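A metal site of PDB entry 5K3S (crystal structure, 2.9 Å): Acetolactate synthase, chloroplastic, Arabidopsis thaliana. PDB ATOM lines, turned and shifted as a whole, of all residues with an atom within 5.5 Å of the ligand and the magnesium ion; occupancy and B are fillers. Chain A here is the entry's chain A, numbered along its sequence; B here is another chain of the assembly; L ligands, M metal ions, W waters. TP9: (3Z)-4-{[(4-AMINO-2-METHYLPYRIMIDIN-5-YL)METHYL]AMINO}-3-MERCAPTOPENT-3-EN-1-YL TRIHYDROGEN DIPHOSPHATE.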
ATOM      1  N   VAL A 400      16.777 -13.726   5.818  1.00  0.00           N
ATOM      2  CA  VAL A 400      17.781 -13.690   6.866  1.00  0.00           C
ATOM      3  C   VAL A 400      17.947 -12.275   7.412  1.00  0.00           C
ATOM      4  O   VAL A 400      18.095 -11.316   6.651  1.00  0.00           O
ATOM      5  CB  VAL A 400      19.141 -14.214   6.372  1.00  0.00           C
ATOM      6  CG1 VAL A 400      20.227 -13.987   7.410  1.00  0.00           C
ATOM      7  CG2 VAL A 400      19.038 -15.689   6.020  1.00  0.00           C
ATOM      8  N   GLY A 401      17.905 -12.146   8.731  1.00  0.00           N
ATOM      9  CA  GLY A 401      18.064 -10.853   9.383  1.00  0.00           C
ATOM     10  C   GLY A 401      17.237 -10.706  10.637  1.00  0.00           C
ATOM     11  O   GLY A 401      16.938 -11.700  11.307  1.00  0.00           O
ATOM     12  N   GLN A 402      16.867  -9.479  10.951  1.00  0.00           N
ATOM     13  CA  GLN A 402      16.045  -9.193  12.116  1.00  0.00           C
ATOM     14  C   GLN A 402      14.687  -9.886  12.033  1.00  0.00           C
ATOM     15  O   GLN A 402      14.215 -10.461  13.012  1.00  0.00           O
ATOM     16  CB  GLN A 402      15.850  -7.680  12.285  1.00  0.00           C
ATOM     17  CG  GLN A 402      17.085  -6.930  12.718  1.00  0.00           C
ATOM     18  CD  GLN A 402      16.820  -5.453  12.915  1.00  0.00           C
ATOM     19  OE1 GLN A 402      15.977  -4.867  12.245  1.00  0.00           O
ATOM     20  NE2 GLN A 402      17.550  -4.835  13.847  1.00  0.00           N
ATOM     21  N   HIS A 403      14.073  -9.817  10.857  1.00  0.00           N
ATOM     22  CA  HIS A 403      12.761 -10.410  10.634  1.00  0.00           C
ATOM     23  C   HIS A 403      12.813 -11.922  10.822  1.00  0.00           C
ATOM     24  O   HIS A 403      11.826 -12.539  11.242  1.00  0.00           O
ATOM     25  CB  HIS A 403      12.244 -10.076   9.230  1.00  0.00           C
ATOM     26  CG  HIS A 403      12.990 -10.765   8.134  1.00  0.00           C
ATOM     27  ND1 HIS A 403      14.223 -10.331   7.675  1.00  0.00           N
ATOM     28  CD2 HIS A 403      12.686 -11.865   7.408  1.00  0.00           C
ATOM     29  CE1 HIS A 403      14.633 -11.136   6.714  1.00  0.00           C
ATOM     30  NE2 HIS A 403      13.724 -12.073   6.529  1.00  0.00           N
ATOM     31  N   GLN A 404      13.963 -12.518  10.514  1.00  0.00           N
ATOM     32  CA  GLN A 404      14.152 -13.956  10.667  1.00  0.00           C
ATOM     33  C   GLN A 404      14.092 -14.355  12.140  1.00  0.00           C
ATOM     34  O   GLN A 404      13.483 -15.372  12.492  1.00  0.00           O
ATOM     35  CB  GLN A 404      15.475 -14.387  10.054  1.00  0.00           C
ATOM     36  CG  GLN A 404      15.745 -15.882  10.142  1.00  0.00           C
ATOM     37  CD  GLN A 404      17.162 -16.244   9.742  1.00  0.00           C
ATOM     38  OE1 GLN A 404      18.043 -15.376   9.683  1.00  0.00           O
ATOM     39  NE2 GLN A 404      17.396 -17.513   9.452  1.00  0.00           N
ATOM     40  N   TRP A 406      12.714 -12.601  14.704  1.00  0.00           N
ATOM     41  CA  TRP A 406      11.381 -12.333  15.241  1.00  0.00           C
ATOM     42  C   TRP A 406      10.385 -13.391  14.784  1.00  0.00           C
ATOM     43  O   TRP A 406       9.461 -13.727  15.527  1.00  0.00           O
ATOM     44  CB  TRP A 406      10.914 -10.932  14.824  1.00  0.00           C
ATOM     45  CG  TRP A 406      11.695  -9.836  15.466  1.00  0.00           C
ATOM     46  CD1 TRP A 406      12.177  -9.808  16.744  1.00  0.00           C
ATOM     47  CD2 TRP A 406      12.111  -8.610  14.857  1.00  0.00           C
ATOM     48  NE1 TRP A 406      12.844  -8.630  16.977  1.00  0.00           N
ATOM     49  CE2 TRP A 406      12.832  -7.877  15.832  1.00  0.00           C
ATOM     50  CE3 TRP A 406      11.950  -8.045  13.585  1.00  0.00           C
ATOM     51  CZ2 TRP A 406      13.368  -6.622  15.568  1.00  0.00           C
ATOM     52  CZ3 TRP A 406      12.491  -6.798  13.332  1.00  0.00           C
ATOM     53  CH2 TRP A 406      13.194  -6.102  14.322  1.00  0.00           C
ATOM     54  N   LEU A 425      24.220 -21.360   6.777  1.00  0.00           N
ATOM     55  CA  LEU A 425      24.759 -20.410   5.807  1.00  0.00           C
ATOM     56  C   LEU A 425      24.115 -19.040   5.981  1.00  0.00           C
ATOM     57  O   LEU A 425      24.760 -18.012   5.779  1.00  0.00           O
ATOM     58  CB  LEU A 425      24.537 -20.926   4.378  1.00  0.00           C
ATOM     59  CG  LEU A 425      25.260 -20.164   3.264  1.00  0.00           C
ATOM     60  CD1 LEU A 425      26.771 -20.310   3.403  1.00  0.00           C
ATOM     61  CD2 LEU A 425      24.795 -20.657   1.893  1.00  0.00           C
ATOM     62  N   GLY A 426      22.838 -19.033   6.348  1.00  0.00           N
ATOM     63  CA  GLY A 426      22.094 -17.794   6.521  1.00  0.00           C
ATOM     64  C   GLY A 426      22.056 -16.985   5.238  1.00  0.00           C
ATOM     65  O   GLY A 426      22.541 -15.855   5.184  1.00  0.00           O
ATOM     66  N   ALA A 427      21.460 -17.567   4.202  1.00  0.00           N
ATOM     67  CA  ALA A 427      21.427 -16.942   2.886  1.00  0.00           C
ATOM     68  C   ALA A 427      20.165 -16.117   2.663  1.00  0.00           C
ATOM     69  O   ALA A 427      19.058 -16.638   2.776  1.00  0.00           O
ATOM     70  CB  ALA A 427      21.564 -17.999   1.798  1.00  0.00           C
ATOM     71  N   MET A 428      20.345 -14.839   2.358  1.00  0.00           N
ATOM     72  CA  MET A 428      19.226 -13.969   2.004  1.00  0.00           C
ATOM     73  C   MET A 428      18.584 -14.432   0.696  1.00  0.00           C
ATOM     74  O   MET A 428      19.210 -15.117  -0.099  1.00  0.00           O
ATOM     75  CB  MET A 428      19.683 -12.520   1.893  1.00  0.00           C
ATOM     76  CG  MET A 428      20.076 -11.884   3.213  1.00  0.00           C
ATOM     77  SD  MET A 428      20.814 -10.253   2.988  1.00  0.00           S
ATOM     78  CE  MET A 428      19.510  -9.423   2.081  1.00  0.00           C
ATOM     79  N   GLY A 452      12.298  -9.968   4.719  1.00  0.00           N
ATOM     80  CA  GLY A 452      12.804  -8.612   4.899  1.00  0.00           C
ATOM     81  C   GLY A 452      12.916  -7.936   3.556  1.00  0.00           C
ATOM     82  O   GLY A 452      13.028  -8.613   2.530  1.00  0.00           O
ATOM     83  N   ASP A 453      12.883  -6.613   3.539  1.00  0.00           N
ATOM     84  CA  ASP A 453      12.889  -5.860   2.279  1.00  0.00           C
ATOM     85  C   ASP A 453      14.165  -6.073   1.479  1.00  0.00           C
ATOM     86  O   ASP A 453      14.159  -5.945   0.255  1.00  0.00           O
ATOM     87  CB  ASP A 453      12.690  -4.365   2.552  1.00  0.00           C
ATOM     88  CG  ASP A 453      13.726  -3.805   3.507  1.00  0.00           C
ATOM     89  OD1 ASP A 453      14.069  -4.487   4.490  1.00  0.00           O
ATOM     90  OD2 ASP A 453      14.193  -2.671   3.258  1.00  0.00           O
ATOM     91  N   GLY A 454      15.249  -6.404   2.166  1.00  0.00           N
ATOM     92  CA  GLY A 454      16.507  -6.697   1.503  1.00  0.00           C
ATOM     93  C   GLY A 454      16.526  -8.117   0.959  1.00  0.00           C
ATOM     94  O   GLY A 454      16.964  -8.352  -0.172  1.00  0.00           O
ATOM     95  N   SER A 455      16.054  -9.060   1.768  1.00  0.00           N
ATOM     96  CA  SER A 455      16.035 -10.465   1.382  1.00  0.00           C
ATOM     97  C   SER A 455      15.008 -10.726   0.289  1.00  0.00           C
ATOM     98  O   SER A 455      15.246 -11.529  -0.615  1.00  0.00           O
ATOM     99  CB  SER A 455      15.754 -11.342   2.598  1.00  0.00           C
ATOM    100  OG  SER A 455      16.721 -11.143   3.615  1.00  0.00           O
ATOM    101  N   PHE A 456      13.879 -10.046   0.374  1.00  0.00           N
ATOM    102  CA  PHE A 456      12.779 -10.253  -0.563  1.00  0.00           C
ATOM    103  C   PHE A 456      13.141  -9.831  -1.989  1.00  0.00           C
ATOM    104  O   PHE A 456      12.771 -10.515  -2.947  1.00  0.00           O
ATOM    105  CB  PHE A 456      11.536  -9.482  -0.104  1.00  0.00           C
ATOM    106  CG  PHE A 456      10.370  -9.578  -1.043  1.00  0.00           C
ATOM    107  CD1 PHE A 456       9.623 -10.748  -1.126  1.00  0.00           C
ATOM    108  CD2 PHE A 456      10.024  -8.513  -1.852  1.00  0.00           C
ATOM    109  CE1 PHE A 456       8.549 -10.840  -1.994  1.00  0.00           C
ATOM    110  CE2 PHE A 456       8.959  -8.594  -2.726  1.00  0.00           C
ATOM    111  CZ  PHE A 456       8.214  -9.760  -2.795  1.00  0.00           C
ATOM    112  N   MET A 458      16.038  -9.724  -3.456  1.00  0.00           N
ATOM    113  CA  MET A 458      17.115 -10.496  -4.070  1.00  0.00           C
ATOM    114  C   MET A 458      16.597 -11.518  -5.078  1.00  0.00           C
ATOM    115  O   MET A 458      17.160 -11.662  -6.166  1.00  0.00           O
ATOM    116  CB  MET A 458      17.944 -11.220  -3.001  1.00  0.00           C
ATOM    117  CG  MET A 458      18.970 -10.327  -2.315  1.00  0.00           C
ATOM    118  SD  MET A 458      20.297 -11.290  -1.552  1.00  0.00           S
ATOM    119  CE  MET A 458      21.419  -9.992  -1.061  1.00  0.00           C
ATOM    120  N   LEU A 478       8.127  -7.633   6.202  1.00  0.00           N
ATOM    121  CA  LEU A 478       8.463  -6.690   7.260  1.00  0.00           C
ATOM    122  C   LEU A 478       9.459  -5.667   6.724  1.00  0.00           C
ATOM    123  O   LEU A 478      10.660  -5.930   6.662  1.00  0.00           O
ATOM    124  CB  LEU A 478       9.036  -7.406   8.477  1.00  0.00           C
ATOM    125  CG  LEU A 478       8.133  -8.469   9.115  1.00  0.00           C
ATOM    126  CD1 LEU A 478       8.737  -8.995  10.404  1.00  0.00           C
ATOM    127  CD2 LEU A 478       6.734  -7.917   9.347  1.00  0.00           C
ATOM    128  N   ASN A 480      11.615  -2.443   6.850  1.00  0.00           N
ATOM    129  CA  ASN A 480      12.257  -1.456   7.705  1.00  0.00           C
ATOM    130  C   ASN A 480      13.189  -0.536   6.911  1.00  0.00           C
ATOM    131  O   ASN A 480      13.946   0.233   7.499  1.00  0.00           O
ATOM    132  CB  ASN A 480      13.033  -2.138   8.833  1.00  0.00           C
ATOM    133  CG  ASN A 480      14.005  -3.193   8.326  1.00  0.00           C
ATOM    134  OD1 ASN A 480      14.291  -3.275   7.127  1.00  0.00           O
ATOM    135  ND2 ASN A 480      14.531  -3.999   9.240  1.00  0.00           N
ATOM    136  N   GLN A 481      13.136  -0.656   5.592  1.00  0.00           N
ATOM    137  CA  GLN A 481      13.928   0.171   4.681  1.00  0.00           C
ATOM    138  C   GLN A 481      15.432   0.038   4.922  1.00  0.00           C
ATOM    139  O   GLN A 481      16.210   0.898   4.508  1.00  0.00           O
ATOM    140  CB  GLN A 481      13.518   1.638   4.786  1.00  0.00           C
ATOM    141  CG  GLN A 481      12.080   1.923   4.362  1.00  0.00           C
ATOM    142  CD  GLN A 481      11.894   1.823   2.863  1.00  0.00           C
ATOM    143  OE1 GLN A 481      12.039   2.803   2.140  1.00  0.00           O
ATOM    144  NE2 GLN A 481      11.551   0.622   2.381  1.00  0.00           N
ATOM    145  N   HIS A 482      15.834  -1.033   5.584  1.00  0.00           N
ATOM    146  CA  HIS A 482      17.236  -1.225   5.956  1.00  0.00           C
ATOM    147  C   HIS A 482      17.660  -2.679   5.906  1.00  0.00           C
ATOM    148  O   HIS A 482      16.835  -3.588   5.807  1.00  0.00           O
ATOM    149  CB  HIS A 482      17.502  -0.688   7.365  1.00  0.00           C
ATOM    150  CG  HIS A 482      17.602   0.812   7.443  1.00  0.00           C
ATOM    151  ND1 HIS A 482      16.495   1.631   7.424  1.00  0.00           N
ATOM    152  CD2 HIS A 482      18.671   1.625   7.540  1.00  0.00           C
ATOM    153  CE1 HIS A 482      16.879   2.892   7.516  1.00  0.00           C
ATOM    154  NE2 HIS A 482      18.201   2.916   7.579  1.00  0.00           N
ATOM    155  N   LEU A 483      18.977  -2.898   5.958  1.00  0.00           N
ATOM    156  CA  LEU A 483      19.515  -4.217   6.238  1.00  0.00           C
ATOM    157  C   LEU A 483      19.626  -4.345   7.760  1.00  0.00           C
ATOM    158  O   LEU A 483      20.712  -4.265   8.329  1.00  0.00           O
ATOM    159  CB  LEU A 483      20.878  -4.404   5.571  1.00  0.00           C
ATOM    160  CG  LEU A 483      20.899  -4.320   4.042  1.00  0.00           C
ATOM    161  CD1 LEU A 483      22.313  -4.379   3.511  1.00  0.00           C
ATOM    162  CD2 LEU A 483      20.054  -5.427   3.427  1.00  0.00           C
ATOM    163  N   GLY A 484      18.471  -4.542   8.390  1.00  0.00           N
ATOM    164  CA  GLY A 484      18.316  -4.436   9.836  1.00  0.00           C
ATOM    165  C   GLY A 484      19.366  -5.092  10.710  1.00  0.00           C
ATOM    166  O   GLY A 484      19.848  -4.464  11.661  1.00  0.00           O
ATOM    167  N   MET A 485      19.708  -6.336  10.413  1.00  0.00           N
ATOM    168  CA  MET A 485      20.656  -7.089  11.229  1.00  0.00           C
ATOM    169  C   MET A 485      22.023  -6.408  11.277  1.00  0.00           C
ATOM    170  O   MET A 485      22.605  -6.258  12.342  1.00  0.00           O
ATOM    171  CB  MET A 485      20.794  -8.516  10.696  1.00  0.00           C
ATOM    172  CG  MET A 485      21.602  -9.452  11.601  1.00  0.00           C
ATOM    173  SD  MET A 485      20.695 -10.005  13.054  1.00  0.00           S
ATOM    174  CE  MET A 485      21.185  -8.792  14.278  1.00  0.00           C
ATOM    175  N   VAL A 486      22.523  -6.000  10.113  1.00  0.00           N
ATOM    176  CA  VAL A 486      23.789  -5.296  10.029  1.00  0.00           C
ATOM    177  C   VAL A 486      23.662  -3.915  10.675  1.00  0.00           C
ATOM    178  O   VAL A 486      24.575  -3.441  11.343  1.00  0.00           O
ATOM    179  CB  VAL A 486      24.261  -5.138   8.564  1.00  0.00           C
ATOM    180  CG1 VAL A 486      25.600  -4.416   8.503  1.00  0.00           C
ATOM    181  CG2 VAL A 486      24.355  -6.500   7.900  1.00  0.00           C
ATOM    182  N   LEU A 503      18.307   0.980   2.366  1.00  0.00           N
ATOM    183  CA  LEU A 503      17.866   0.393   1.109  1.00  0.00           C
ATOM    184  C   LEU A 503      16.911   1.292   0.325  1.00  0.00           C
ATOM    185  O   LEU A 503      16.521   0.967  -0.798  1.00  0.00           O
ATOM    186  CB  LEU A 503      17.199  -0.955   1.360  1.00  0.00           C
ATOM    187  CG  LEU A 503      18.085  -2.030   1.973  1.00  0.00           C
ATOM    188  CD1 LEU A 503      17.284  -3.303   2.229  1.00  0.00           C
ATOM    189  CD2 LEU A 503      19.275  -2.327   1.071  1.00  0.00           C
ATOM    190  N   TYR B  33      28.553  -5.227  -0.984  1.00  0.00           N
ATOM    191  CA  TYR B  33      27.311  -5.536  -0.267  1.00  0.00           C
ATOM    192  C   TYR B  33      27.657  -6.031   1.132  1.00  0.00           C
ATOM    193  O   TYR B  33      28.271  -7.091   1.288  1.00  0.00           O
ATOM    194  CB  TYR B  33      26.501  -6.579  -1.037  1.00  0.00           C
ATOM    195  CG  TYR B  33      25.047  -6.660  -0.610  1.00  0.00           C
ATOM    196  CD1 TYR B  33      24.667  -7.425   0.479  1.00  0.00           C
ATOM    197  CD2 TYR B  33      24.062  -5.966  -1.302  1.00  0.00           C
ATOM    198  CE1 TYR B  33      23.338  -7.501   0.867  1.00  0.00           C
ATOM    199  CE2 TYR B  33      22.741  -6.031  -0.920  1.00  0.00           C
ATOM    200  CZ  TYR B  33      22.380  -6.805   0.163  1.00  0.00           C
ATOM    201  OH  TYR B  33      21.059  -6.871   0.546  1.00  0.00           O
ATOM    202  N   PRO B  34      27.255  -5.269   2.161  1.00  0.00           N
ATOM    203  CA  PRO B  34      27.683  -5.507   3.548  1.00  0.00           C
ATOM    204  C   PRO B  34      27.152  -6.803   4.158  1.00  0.00           C
ATOM    205  O   PRO B  34      26.131  -7.334   3.743  1.00  0.00           O
ATOM    206  CB  PRO B  34      27.101  -4.305   4.297  1.00  0.00           C
ATOM    207  CG  PRO B  34      25.937  -3.888   3.484  1.00  0.00           C
ATOM    208  CD  PRO B  34      26.322  -4.135   2.061  1.00  0.00           C
ATOM    209  N   GLY B  35      27.887  -7.300   5.149  1.00  0.00           N
ATOM    210  CA  GLY B  35      27.505  -8.470   5.900  1.00  0.00           C
ATOM    211  C   GLY B  35      28.347  -8.553   7.161  1.00  0.00           C
ATOM    212  O   GLY B  35      29.335  -7.824   7.290  1.00  0.00           O
ATOM    213  N   GLY B  36      27.965  -9.422   8.084  1.00  0.00           N
ATOM    214  CA  GLY B  36      28.623  -9.528   9.367  1.00  0.00           C
ATOM    215  C   GLY B  36      30.126  -9.722   9.320  1.00  0.00           C
ATOM    216  O   GLY B  36      30.861  -9.183  10.151  1.00  0.00           O
ATOM    217  N   GLU B  59      24.711  -9.741  -4.719  1.00  0.00           N
ATOM    218  CA  GLU B  59      26.153  -9.821  -4.966  1.00  0.00           C
ATOM    219  C   GLU B  59      26.473 -10.210  -6.414  1.00  0.00           C
ATOM    220  O   GLU B  59      27.496  -9.803  -6.952  1.00  0.00           O
ATOM    221  CB  GLU B  59      26.814 -10.808  -4.010  1.00  0.00           C
ATOM    222  CG  GLU B  59      26.936 -10.306  -2.580  1.00  0.00           C
ATOM    223  CD  GLU B  59      25.729 -10.660  -1.729  1.00  0.00           C
ATOM    224  OE1 GLU B  59      24.721 -11.155  -2.295  1.00  0.00           O
ATOM    225  OE2 GLU B  59      25.795 -10.458  -0.502  1.00  0.00           O
ATOM    226  N   THR B  82      30.335 -10.354   1.715  1.00  0.00           N
ATOM    227  CA  THR B  82      30.590 -10.956   3.012  1.00  0.00           C
ATOM    228  C   THR B  82      30.845 -12.452   2.860  1.00  0.00           C
ATOM    229  O   THR B  82      30.829 -12.982   1.752  1.00  0.00           O
ATOM    230  CB  THR B  82      29.417 -10.738   3.986  1.00  0.00           C
ATOM    231  OG1 THR B  82      29.792 -11.179   5.301  1.00  0.00           O
ATOM    232  CG2 THR B  82      28.179 -11.499   3.528  1.00  0.00           C
ATOM    233  N   PRO B  85      27.119 -16.923   2.119  1.00  0.00           N
ATOM    234  CA  PRO B  85      26.142 -16.660   1.052  1.00  0.00           C
ATOM    235  C   PRO B  85      26.519 -15.472   0.181  1.00  0.00           C
ATOM    236  O   PRO B  85      26.190 -15.445  -0.999  1.00  0.00           O
ATOM    237  CB  PRO B  85      24.845 -16.380   1.829  1.00  0.00           C
ATOM    238  CG  PRO B  85      25.306 -15.902   3.161  1.00  0.00           C
ATOM    239  CD  PRO B  85      26.543 -16.696   3.451  1.00  0.00           C
ATOM    240  N   GLY B  86      27.216 -14.499   0.763  1.00  0.00           N
ATOM    241  CA  GLY B  86      27.679 -13.357   0.013  1.00  0.00           C
ATOM    242  C   GLY B  86      28.736 -13.768  -1.000  1.00  0.00           C
ATOM    243  O   GLY B  86      28.712 -13.349  -2.152  1.00  0.00           O
ATOM    244  N   ASN B  89      27.501 -15.982  -3.961  1.00  0.00           N
ATOM    245  CA  ASN B  89      26.726 -15.236  -4.946  1.00  0.00           C
ATOM    246  C   ASN B  89      27.632 -14.549  -5.978  1.00  0.00           C
ATOM    247  O   ASN B  89      27.140 -13.961  -6.947  1.00  0.00           O
ATOM    248  CB  ASN B  89      25.843 -14.194  -4.263  1.00  0.00           C
ATOM    249  CG  ASN B  89      24.547 -14.798  -3.735  1.00  0.00           C
ATOM    250  OD1 ASN B  89      24.150 -15.888  -4.137  1.00  0.00           O
ATOM    251  ND2 ASN B  89      23.883 -14.076  -2.843  1.00  0.00           N
ATOM    252  N   GLN B 122      27.986 -18.826   8.653  1.00  0.00           N
ATOM    253  CA  GLN B 122      28.229 -18.238   7.334  1.00  0.00           C
ATOM    254  C   GLN B 122      29.643 -18.510   6.826  1.00  0.00           C
ATOM    255  O   GLN B 122      30.265 -17.642   6.231  1.00  0.00           O
ATOM    256  CB  GLN B 122      27.966 -16.728   7.353  1.00  0.00           C
ATOM    257  CG  GLN B 122      26.550 -16.350   7.747  1.00  0.00           C
ATOM    258  CD  GLN B 122      26.224 -14.913   7.406  1.00  0.00           C
ATOM    259  OE1 GLN B 122      25.124 -14.610   6.928  1.00  0.00           O
ATOM    260  NE2 GLN B 122      27.171 -14.015   7.638  1.00  0.00           N
HETATM  261  N1' TP9 L   1      23.986 -11.636   1.357  1.00  0.00           N
HETATM  262  C2' TP9 L   1      23.357 -12.770   1.588  1.00  0.00           C
HETATM  263  CM2 TP9 L   1      22.914 -13.596   0.402  1.00  0.00           C
HETATM  264  N3' TP9 L   1      23.094 -13.205   2.802  1.00  0.00           N
HETATM  265  C4' TP9 L   1      23.465 -12.496   3.880  1.00  0.00           C
HETATM  266  N4' TP9 L   1      23.169 -12.989   5.187  1.00  0.00           N
HETATM  267  C5' TP9 L   1      24.149 -11.279   3.696  1.00  0.00           C
HETATM  268  C6' TP9 L   1      24.397 -10.868   2.379  1.00  0.00           C
HETATM  269  C7' TP9 L   1      24.608 -10.421   4.854  1.00  0.00           C
HETATM  270  N3  TP9 L   1      23.577 -10.222   5.811  1.00  0.00           N
HETATM  271  S1  TP9 L   1      20.980 -10.342   7.557  1.00  0.00           S
HETATM  272  C5  TP9 L   1      21.516  -9.078   6.437  1.00  0.00           C
HETATM  273  C4  TP9 L   1      22.668  -9.133   5.739  1.00  0.00           C
HETATM  274  CM4 TP9 L   1      23.151  -8.072   4.781  1.00  0.00           C
HETATM  275  C6  TP9 L   1      20.507  -7.946   6.407  1.00  0.00           C
HETATM  276  C7  TP9 L   1      19.273  -8.291   5.587  1.00  0.00           C
HETATM  277  O7  TP9 L   1      18.266  -7.354   5.899  1.00  0.00           O
HETATM  278  PA  TP9 L   1      16.759  -7.711   5.562  1.00  0.00           P
HETATM  279  O1A TP9 L   1      16.717  -8.826   4.531  1.00  0.00           O
HETATM  280  O2A TP9 L   1      16.053  -6.501   5.015  1.00  0.00           O
HETATM  281  O3A TP9 L   1      16.046  -8.184   6.881  1.00  0.00           O
HETATM  282  PB  TP9 L   1      16.037  -7.325   8.214  1.00  0.00           P
HETATM  283  O1B TP9 L   1      17.210  -7.737   9.078  1.00  0.00           O
HETATM  284  O2B TP9 L   1      16.165  -5.857   7.870  1.00  0.00           O
HETATM  285  O3B TP9 L   1      14.750  -7.555   8.962  1.00  0.00           O
HETATM  286 MG    MG M   1      15.242  -4.912   6.197  1.00  0.00          MG
HETATM  287  O   HOH W   1      13.436  -5.957   6.881  1.00  0.00           O
HETATM  288  O   HOH W   2      24.192 -10.364   8.751  1.00  0.00           O
HETATM  289  O   HOH W   3      21.218 -15.205  -2.004  1.00  0.00           O
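Gly 452 touches the ligand (C to O2A, 3.7 Å).
CE of Met 458 touches N1' of the ligand, 3.9 Å away.
CA of Leu 483 touches O7 of the ligand, 3.4 Å away.
Val 486 touches the ligand (CG2 to CM4, 3.7 Å).
CE1 of Tyr 33 of chain B touches C6' of the ligand, at 3.8 Å.
Pro 34 of chain B touches the ligand.
Gly 35 of chain B touches the ligand (CA to C7', 3.6 Å).
Thr 82 of chain B touches the ligand.
Pro 85 of chain B touches the ligand.
Asn 89 of chain B touches the ligand.
Of the 35 residues printed, 25 come within 4 Å of the ligand.
N of Gly 484 touches the magnesium ion (3.9 Å).
Within 4 Å of the magnesium ion: Asp 453, Asn 480, His 482 and Gly 484.
An oxygen (O3A) of the ligand sits at hydrogen-bond distance from a ring nitrogen (ND1) of His 403 (2.9 Å).
The backbone NH of Met 428 sits at hydrogen-bond distance from a nitrogen (N3') of the ligand (3.2 Å).
O1A of the ligand sits at hydrogen-bond distance from OG of Ser 455, 2.5 Å away.
The backbone carbonyl oxygen (O) of Gly 426 lies within hydrogen-bond range of a nitrogen (N4') of the ligand, at 2.9 Å.
A sulfur (S1) of the ligand lies close to the backbone NH (N) of Gly 401, at 3.8 Å.
The backbone NH (N) of Met 485 lies within hydrogen-bond range of an oxygen (O1B) of the ligand (3.2 Å).
The backbone NH (N) of Ser 455 lies within hydrogen-bond range of an oxygen (O1A) of the ligand, at 2.9 Å.
The side-chain amide oxygen (OE1) of Gln 122 of chain B lies within hydrogen-bond range of a nitrogen (N4') of the ligand (3.1 Å).
The backbone NH (N) of Gln 402 sits at hydrogen-bond distance from an oxygen (O1B) of the ligand, 2.6 Å away.
A nitrogen (N1') of the ligand sits at hydrogen-bond distance from the side-chain carboxylate (OE2) of Glu 59 of chain B (2.8 Å).
An oxygen (O3B) of the ligand sits at hydrogen-bond distance from the backbone NH (N) of His 403 (3.0 Å).
N of Gly 484 lies close to O2B of the ligand (2.7 Å).
O of Val 400 lies close to S1 of the ligand (3.2 Å).
The backbone NH (N) of Gly 454 lies close to an oxygen (O2A) of the ligand, 3.0 Å away.
O2A of the ligand lies close to N of Asp 453 (3.5 Å).
The magnesium ion is bound by O of His 482.
The side-chain amide oxygen (OD1) of Asn 480 is bound to the magnesium ion.
OD1 of Asp 453 is bound to the magnesium ion (2.1 Å).
The magnesium ion is bound by an oxygen (O2B) of the ligand, at 2.1 Å.
An oxygen (O2A) of the ligand binds the magnesium ion, 2.1 Å away.
Water W1 is bound to the magnesium ion (2.2 Å).
The magnesium ion has six donor atoms within binding distance.
Water W1 lies within hydrogen-bond range of O of Leu 478 (2.8 Å), O3B of the ligand (2.9 Å), ND2 of Asn 480 (3.3 Å) and N of Asp 453 (3.5 Å).
Water W3 bridges O of Met 428 (2.8 Å) and ND2 of Asn 89 of chain B (3.0 Å).
ND2 of Asn 480 sits at hydrogen-bond distance from OE1 of Gln 402, at 3.4 Å.
The side-chain amide oxygen (OE1) of Gln 404 is in hydrogen-bond range of the backbone NH (N) of Gly 401, at 3.4 Å.
O of Gly 484 lies within hydrogen-bond range of NE2 of Gln 402 (3.2 Å).
OD2 of Asp 453 sits close to N of Gln 481.
A ring nitrogen (NE2) of His 403 lies within hydrogen-bond range of the backbone NH (N) of Gly 452 (3.1 Å).
OE1 of Gln 122 of chain B lies close to O of Gly 426.
The side-chain amide nitrogen (ND2) of Asn 89 of chain B lies within hydrogen-bond range of the side-chain carboxylate (OE1) of Glu 59 of chain B, at 3.1 Å.
O of Val 400 lies within hydrogen-bond range of OG of Ser 455 (3.3 Å).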
